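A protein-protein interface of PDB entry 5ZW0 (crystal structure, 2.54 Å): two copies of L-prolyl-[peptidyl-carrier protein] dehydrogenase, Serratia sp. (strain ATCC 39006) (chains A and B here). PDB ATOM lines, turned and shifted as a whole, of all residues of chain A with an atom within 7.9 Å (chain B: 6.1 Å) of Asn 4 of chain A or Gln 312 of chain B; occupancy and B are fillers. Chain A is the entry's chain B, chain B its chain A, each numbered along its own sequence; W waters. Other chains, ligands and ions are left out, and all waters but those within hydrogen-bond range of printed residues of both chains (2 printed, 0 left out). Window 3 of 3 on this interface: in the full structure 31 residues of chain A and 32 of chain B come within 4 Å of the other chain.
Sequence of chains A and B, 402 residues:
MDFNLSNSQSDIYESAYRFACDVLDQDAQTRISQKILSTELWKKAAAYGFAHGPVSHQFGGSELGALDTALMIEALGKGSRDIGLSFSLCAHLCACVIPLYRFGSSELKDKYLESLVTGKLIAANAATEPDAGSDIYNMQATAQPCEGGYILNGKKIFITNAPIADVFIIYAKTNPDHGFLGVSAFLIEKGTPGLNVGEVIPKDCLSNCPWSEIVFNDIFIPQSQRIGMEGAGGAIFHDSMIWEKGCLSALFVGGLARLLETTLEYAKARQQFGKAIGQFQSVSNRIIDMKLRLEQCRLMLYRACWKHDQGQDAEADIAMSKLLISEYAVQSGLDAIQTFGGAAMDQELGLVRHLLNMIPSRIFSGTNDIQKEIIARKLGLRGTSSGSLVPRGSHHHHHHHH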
ATOM      1  N   MET A   1      10.160   7.561  24.287  1.00  0.00           N
ATOM      2  CA  MET A   1       9.931   6.388  23.459  1.00  0.00           C
ATOM      3  C   MET A   1      11.219   5.608  23.223  1.00  0.00           C
ATOM      4  O   MET A   1      12.215   6.159  22.770  1.00  0.00           O
ATOM      5  CB  MET A   1       9.317   6.799  22.141  1.00  0.00           C
ATOM      6  CG  MET A   1       8.584   5.675  21.457  1.00  0.00           C
ATOM      7  SD  MET A   1       6.945   6.219  20.972  1.00  0.00           S
ATOM      8  CE  MET A   1       5.950   4.915  21.698  1.00  0.00           C
ATOM      9  N   ASP A   2      11.199   4.322  23.556  1.00  0.00           N
ATOM     10  CA  ASP A   2      12.387   3.484  23.509  1.00  0.00           C
ATOM     11  C   ASP A   2      11.918   2.059  23.268  1.00  0.00           C
ATOM     12  O   ASP A   2      10.976   1.603  23.919  1.00  0.00           O
ATOM     13  CB  ASP A   2      13.179   3.583  24.828  1.00  0.00           C
ATOM     14  CG  ASP A   2      14.474   2.765  24.807  1.00  0.00           C
ATOM     15  OD1 ASP A   2      15.543   3.406  24.898  1.00  0.00           O
ATOM     16  OD2 ASP A   2      14.455   1.514  24.680  1.00  0.00           O
ATOM     17  N   PHE A   3      12.570   1.343  22.360  1.00  0.00           N
ATOM     18  CA  PHE A   3      12.075   0.022  21.996  1.00  0.00           C
ATOM     19  C   PHE A   3      13.079  -1.076  22.301  1.00  0.00           C
ATOM     20  O   PHE A   3      12.976  -2.184  21.752  1.00  0.00           O
ATOM     21  CB  PHE A   3      11.657  -0.016  20.520  1.00  0.00           C
ATOM     22  CG  PHE A   3      10.428   0.809  20.219  1.00  0.00           C
ATOM     23  CD1 PHE A   3       9.169   0.276  20.387  1.00  0.00           C
ATOM     24  CD2 PHE A   3      10.538   2.114  19.767  1.00  0.00           C
ATOM     25  CE1 PHE A   3       8.038   1.022  20.114  1.00  0.00           C
ATOM     26  CE2 PHE A   3       9.422   2.851  19.492  1.00  0.00           C
ATOM     27  CZ  PHE A   3       8.159   2.303  19.661  1.00  0.00           C
ATOM     28  N   ASN A   4      14.058  -0.788  23.148  1.00  0.00           N
ATOM     29  CA  ASN A   4      14.978  -1.814  23.619  1.00  0.00           C
ATOM     30  C   ASN A   4      14.613  -2.266  25.027  1.00  0.00           C
ATOM     31  O   ASN A   4      14.128  -1.482  25.861  1.00  0.00           O
ATOM     32  CB  ASN A   4      16.433  -1.325  23.586  1.00  0.00           C
ATOM     33  CG  ASN A   4      17.138  -1.681  22.274  1.00  0.00           C
ATOM     34  OD1 ASN A   4      16.709  -2.584  21.554  1.00  0.00           O
ATOM     35  ND2 ASN A   4      18.219  -0.970  21.962  1.00  0.00           N
ATOM     36  N   LEU A   5      14.886  -3.545  25.290  1.00  0.00           N
ATOM     37  CA  LEU A   5      14.851  -4.016  26.663  1.00  0.00           C
ATOM     38  C   LEU A   5      15.953  -3.315  27.447  1.00  0.00           C
ATOM     39  O   LEU A   5      17.102  -3.255  26.998  1.00  0.00           O
ATOM     40  CB  LEU A   5      15.037  -5.539  26.719  1.00  0.00           C
ATOM     41  CG  LEU A   5      14.050  -6.398  25.930  1.00  0.00           C
ATOM     42  CD1 LEU A   5      14.234  -7.864  26.255  1.00  0.00           C
ATOM     43  CD2 LEU A   5      12.606  -5.965  26.177  1.00  0.00           C
ATOM     44  N   SER A   6      15.594  -2.770  28.614  1.00  0.00           N
ATOM     45  CA  SER A   6      16.590  -2.414  29.612  1.00  0.00           C
ATOM     46  C   SER A   6      17.493  -3.622  29.921  1.00  0.00           C
ATOM     47  O   SER A   6      17.135  -4.782  29.642  1.00  0.00           O
ATOM     48  CB  SER A   6      15.912  -1.920  30.892  1.00  0.00           C
ATOM     49  OG  SER A   6      15.418  -2.990  31.697  1.00  0.00           O
ATOM     50  N   ASN A   7      18.673  -3.365  30.501  1.00  0.00           N
ATOM     51  CA  ASN A   7      19.587  -4.464  30.796  1.00  0.00           C
ATOM     52  C   ASN A   7      18.961  -5.445  31.777  1.00  0.00           C
ATOM     53  O   ASN A   7      19.104  -6.662  31.621  1.00  0.00           O
ATOM     54  CB  ASN A   7      20.922  -3.925  31.313  1.00  0.00           C
ATOM     55  CG  ASN A   7      21.728  -3.150  30.231  1.00  0.00           C
ATOM     56  OD1 ASN A   7      21.741  -3.502  29.043  1.00  0.00           O
ATOM     57  ND2 ASN A   7      22.449  -2.131  30.672  1.00  0.00           N
ATOM     58  N   GLN A   9      15.722  -6.111  32.101  1.00  0.00           N
ATOM     59  CA  GLN A   9      14.722  -6.887  31.391  1.00  0.00           C
ATOM     60  C   GLN A   9      15.372  -7.930  30.493  1.00  0.00           C
ATOM     61  O   GLN A   9      14.881  -9.064  30.399  1.00  0.00           O
ATOM     62  CB  GLN A   9      13.825  -5.949  30.585  1.00  0.00           C
ATOM     63  CG  GLN A   9      12.881  -5.157  31.459  1.00  0.00           C
ATOM     64  CD  GLN A   9      12.280  -3.927  30.771  1.00  0.00           C
ATOM     65  OE1 GLN A   9      12.775  -3.451  29.717  1.00  0.00           O
ATOM     66  NE2 GLN A   9      11.234  -3.368  31.404  1.00  0.00           N
ATOM     67  N   SER A  10      16.468  -7.577  29.815  1.00  0.00           N
ATOM     68  CA  SER A  10      17.165  -8.583  29.010  1.00  0.00           C
ATOM     69  C   SER A  10      17.681  -9.696  29.897  1.00  0.00           C
ATOM     70  O   SER A  10      17.671 -10.866  29.506  1.00  0.00           O
ATOM     71  CB  SER A  10      18.320  -7.970  28.218  1.00  0.00           C
ATOM     72  OG  SER A  10      18.166  -6.571  28.214  1.00  0.00           O
ATOM     73  N   LEU A  67       5.562  -5.990  32.907  1.00  0.00           N
ATOM     74  CA  LEU A  67       6.412  -6.235  31.742  1.00  0.00           C
ATOM     75  C   LEU A  67       7.464  -7.294  32.058  1.00  0.00           C
ATOM     76  O   LEU A  67       7.764  -8.154  31.212  1.00  0.00           O
ATOM     77  CB  LEU A  67       7.056  -4.935  31.258  1.00  0.00           C
ATOM     78  CG  LEU A  67       7.869  -5.002  29.963  1.00  0.00           C
ATOM     79  CD1 LEU A  67       7.106  -5.717  28.839  1.00  0.00           C
ATOM     80  CD2 LEU A  67       8.300  -3.628  29.488  1.00  0.00           C
ATOM     81  N   MET B   1      12.524  -0.072  27.580  1.00  0.00           N
ATOM     82  CA  MET B   1      11.210   0.085  26.966  1.00  0.00           C
ATOM     83  C   MET B   1      10.362   1.226  27.546  1.00  0.00           C
ATOM     84  O   MET B   1      10.110   1.276  28.731  1.00  0.00           O
ATOM     85  CB  MET B   1      10.441  -1.218  27.097  1.00  0.00           C
ATOM     86  CG  MET B   1       9.406  -1.394  26.022  1.00  0.00           C
ATOM     87  SD  MET B   1       9.943  -2.631  24.849  1.00  0.00           S
ATOM     88  CE  MET B   1       9.561  -4.051  25.842  1.00  0.00           C
ATOM     89  N   ASP B   2       9.903   2.124  26.687  1.00  0.00           N
ATOM     90  CA  ASP B   2       9.144   3.312  27.067  1.00  0.00           C
ATOM     91  C   ASP B   2       8.202   3.641  25.919  1.00  0.00           C
ATOM     92  O   ASP B   2       8.626   3.655  24.761  1.00  0.00           O
ATOM     93  CB  ASP B   2      10.059   4.520  27.357  1.00  0.00           C
ATOM     94  CG  ASP B   2       9.278   5.820  27.691  1.00  0.00           C
ATOM     95  OD1 ASP B   2       8.176   6.082  27.150  1.00  0.00           O
ATOM     96  OD2 ASP B   2       9.790   6.627  28.492  1.00  0.00           O
ATOM     97  N   TRP B 306      12.570   4.821  15.334  1.00  0.00           N
ATOM     98  CA  TRP B 306      13.460   4.838  16.482  1.00  0.00           C
ATOM     99  C   TRP B 306      14.725   4.036  16.207  1.00  0.00           C
ATOM    100  O   TRP B 306      15.831   4.501  16.500  1.00  0.00           O
ATOM    101  CB  TRP B 306      12.718   4.289  17.686  1.00  0.00           C
ATOM    102  CG  TRP B 306      13.575   4.115  18.906  1.00  0.00           C
ATOM    103  CD1 TRP B 306      13.862   5.064  19.854  1.00  0.00           C
ATOM    104  CD2 TRP B 306      14.223   2.909  19.337  1.00  0.00           C
ATOM    105  NE1 TRP B 306      14.673   4.530  20.824  1.00  0.00           N
ATOM    106  CE2 TRP B 306      14.908   3.208  20.532  1.00  0.00           C
ATOM    107  CE3 TRP B 306      14.318   1.610  18.811  1.00  0.00           C
ATOM    108  CZ2 TRP B 306      15.665   2.243  21.225  1.00  0.00           C
ATOM    109  CZ3 TRP B 306      15.067   0.659  19.499  1.00  0.00           C
ATOM    110  CH2 TRP B 306      15.718   0.977  20.694  1.00  0.00           C
ATOM    111  N   LYS B 307      14.588   2.856  15.597  1.00  0.00           N
ATOM    112  CA  LYS B 307      15.752   2.048  15.236  1.00  0.00           C
ATOM    113  C   LYS B 307      16.714   2.832  14.368  1.00  0.00           C
ATOM    114  O   LYS B 307      17.935   2.784  14.575  1.00  0.00           O
ATOM    115  CB  LYS B 307      15.334   0.790  14.474  1.00  0.00           C
ATOM    116  CG  LYS B 307      14.933  -0.380  15.307  1.00  0.00           C
ATOM    117  CD  LYS B 307      14.854  -1.630  14.433  1.00  0.00           C
ATOM    118  CE  LYS B 307      14.595  -2.871  15.275  1.00  0.00           C
ATOM    119  NZ  LYS B 307      14.146  -4.029  14.459  1.00  0.00           N
ATOM    120  N   HIS B 308      16.183   3.521  13.350  1.00  0.00           N
ATOM    121  CA  HIS B 308      17.036   4.356  12.506  1.00  0.00           C
ATOM    122  C   HIS B 308      17.762   5.415  13.334  1.00  0.00           C
ATOM    123  O   HIS B 308      18.965   5.638  13.164  1.00  0.00           O
ATOM    124  CB  HIS B 308      16.219   5.007  11.406  1.00  0.00           C
ATOM    125  CG  HIS B 308      17.021   5.890  10.509  1.00  0.00           C
ATOM    126  ND1 HIS B 308      17.667   5.417   9.387  1.00  0.00           N
ATOM    127  CD2 HIS B 308      17.262   7.223  10.552  1.00  0.00           C
ATOM    128  CE1 HIS B 308      18.276   6.419   8.780  1.00  0.00           C
ATOM    129  NE2 HIS B 308      18.048   7.527   9.466  1.00  0.00           N
ATOM    130  N   ASP B 309      17.036   6.098  14.220  1.00  0.00           N
ATOM    131  CA  ASP B 309      17.665   7.059  15.114  1.00  0.00           C
ATOM    132  C   ASP B 309      18.740   6.434  16.024  1.00  0.00           C
ATOM    133  O   ASP B 309      19.632   7.151  16.495  1.00  0.00           O
ATOM    134  CB  ASP B 309      16.576   7.752  15.949  1.00  0.00           C
ATOM    135  CG  ASP B 309      15.738   8.731  15.116  1.00  0.00           C
ATOM    136  OD1 ASP B 309      16.127   8.960  13.950  1.00  0.00           O
ATOM    137  OD2 ASP B 309      14.718   9.293  15.613  1.00  0.00           O
ATOM    138  N   GLN B 310      18.694   5.126  16.286  1.00  0.00           N
ATOM    139  CA  GLN B 310      19.753   4.474  17.053  1.00  0.00           C
ATOM    140  C   GLN B 310      20.986   4.145  16.228  1.00  0.00           C
ATOM    141  O   GLN B 310      21.985   3.714  16.798  1.00  0.00           O
ATOM    142  CB  GLN B 310      19.271   3.149  17.647  1.00  0.00           C
ATOM    143  CG  GLN B 310      18.166   3.234  18.635  1.00  0.00           C
ATOM    144  CD  GLN B 310      18.371   4.319  19.635  1.00  0.00           C
ATOM    145  OE1 GLN B 310      17.846   5.412  19.471  1.00  0.00           O
ATOM    146  NE2 GLN B 310      19.128   4.032  20.688  1.00  0.00           N
ATOM    147  N   GLY B 311      20.945   4.315  14.917  1.00  0.00           N
ATOM    148  CA  GLY B 311      21.996   3.814  14.072  1.00  0.00           C
ATOM    149  C   GLY B 311      21.827   2.377  13.643  1.00  0.00           C
ATOM    150  O   GLY B 311      22.615   1.897  12.819  1.00  0.00           O
ATOM    151  N   GLN B 312      20.799   1.687  14.129  1.00  0.00           N
ATOM    152  CA  GLN B 312      20.538   0.329  13.677  1.00  0.00           C
ATOM    153  C   GLN B 312      20.030   0.343  12.233  1.00  0.00           C
ATOM    154  O   GLN B 312      19.686   1.387  11.674  1.00  0.00           O
ATOM    155  CB  GLN B 312      19.542  -0.364  14.611  1.00  0.00           C
ATOM    156  CG  GLN B 312      19.926  -0.257  16.080  1.00  0.00           C
ATOM    157  CD  GLN B 312      18.920  -0.944  16.992  1.00  0.00           C
ATOM    158  OE1 GLN B 312      18.165  -1.825  16.544  1.00  0.00           O
ATOM    159  NE2 GLN B 312      18.921  -0.568  18.287  1.00  0.00           N
ATOM    160  N   ASP B 313      20.031  -0.834  11.606  1.00  0.00           N
ATOM    161  CA  ASP B 313      19.544  -0.968  10.237  1.00  0.00           C
ATOM    162  C   ASP B 313      18.034  -1.188  10.262  1.00  0.00           C
ATOM    163  O   ASP B 313      17.551  -2.204  10.782  1.00  0.00           O
ATOM    164  CB  ASP B 313      20.252  -2.107   9.512  1.00  0.00           C
ATOM    165  CG  ASP B 313      19.586  -2.465   8.210  1.00  0.00           C
ATOM    166  OD1 ASP B 313      19.595  -1.635   7.277  1.00  0.00           O
ATOM    167  OD2 ASP B 313      19.046  -3.587   8.131  1.00  0.00           O
ATOM    168  N   ALA B 314      17.299  -0.243   9.677  1.00  0.00           N
ATOM    169  CA  ALA B 314      15.857  -0.148   9.832  1.00  0.00           C
ATOM    170  C   ALA B 314      15.094  -0.533   8.575  1.00  0.00           C
ATOM    171  O   ALA B 314      13.859  -0.465   8.575  1.00  0.00           O
ATOM    172  CB  ALA B 314      15.485   1.274  10.250  1.00  0.00           C
HETATM  173  O   HOH W   1      16.224   5.961  22.853  1.00  0.00           O
HETATM  174  O   HOH W   2      11.101   0.041  31.125  1.00  0.00           O
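Printed residues of chain B within 4 Å of Phe 3 of chain A: Trp 306. Of chain B, only Met 1, Trp 306 and Gln 312 come within 4 Å of Asn 4 of chain A. Printed residues of chain B within 4 Å of Leu 5 of chain A: Met 1. Of chain A, only Asn 4 comes within 4 Å of Gln 312 of chain B. The nearest residue of chain B that does not touch Asn 4 of chain A is Gln 310 of chain B (5.2 Å). The nearest residue of chain A that does not touch Gln 312 of chain B is Phe 3 of chain A (7.1 Å). The nearest printed residue of chain B that does not touch Leu 67 of chain A is Asp 2 of chain B (6.6 Å).
N of Gln 312 of chain B lies within hydrogen-bond range of O of Lys 307 of chain B (3.1 Å). The backbone NH (N) of Asn 4 of chain A lies within hydrogen-bond range of the side-chain carboxylate (OD2) of Asp 2 of chain A, 2.8 Å away.
Water W2 lies within hydrogen-bond range of O of Met 1 of chain B (2.9 Å) and NE2 of Gln 9 of chain A (3.4 Å). Water W1 bridges the indole nitrogen of Trp 306 of chain B (2.9 Å) and the side-chain carboxylate of Asp 2 of chain A (3.3 Å).
Met 1 of chain A touches Asp 2 of chain B, and with the chains exchanged Asp 2 of chain A touches Met 1 of chain B. Asp 2 of chain B touches its own counterpart, Asp 2 of chain A. Of the 11 pairs that touch across the chains among the printed residues, 3 have their exchanged pair printed and touching as well.
Among the printed residues, pairs that only touch across the chains: Met 1 of chain A with Asp 2 of chain B (3.3 Å), Asn 4 of chain A with Trp 306 of chain B (3.4 Å), Asp 2 of chain A with Met 1 of chain B (3.4 Å), Phe 3 of chain A with Trp 306 of chain B (3.4 Å), Met 1 of chain A with Trp 306 of chain B (3.5 Å), Leu 5 of chain A with Met 1 of chain B (3.6 Å), Asp 2 of chain A with Trp 306 of chain B (3.7 Å), Asn 4 of chain A with Gln 312 of chain B (3.8 Å) and Leu 67 of chain A with Met 1 of chain B (3.9 Å).
The backbone carbonyl oxygen (O) of Asn 4 of chain A is in hydrogen-bond range of the backbone NH (N) of Met 1 of chain B (2.7 Å). N of Asp 2 of chain A lies within hydrogen-bond range of O of Asp 2 of chain B, 2.9 Å away.
Hydrophobic or aromatic side chains of chain A that line the printed part of chain B: Met 1, Phe 3, Leu 5 and Leu 67. Along chain A the printed residues that touch a printed residue of chain B span positions 1 to 67. Of the 11 printed residues of chain B, 4 touch a printed residue of chain A. Printed residues of chain B that touch a printed residue of chain A: Met 1, Asp 2, Trp 306 and Gln 312. Among the printed residues, 11 pairs touch across the chains. Among the printed residues, no Asp or Glu carboxylate lies within 4 Å of a Lys or Arg side-chain nitrogen of the other chain.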
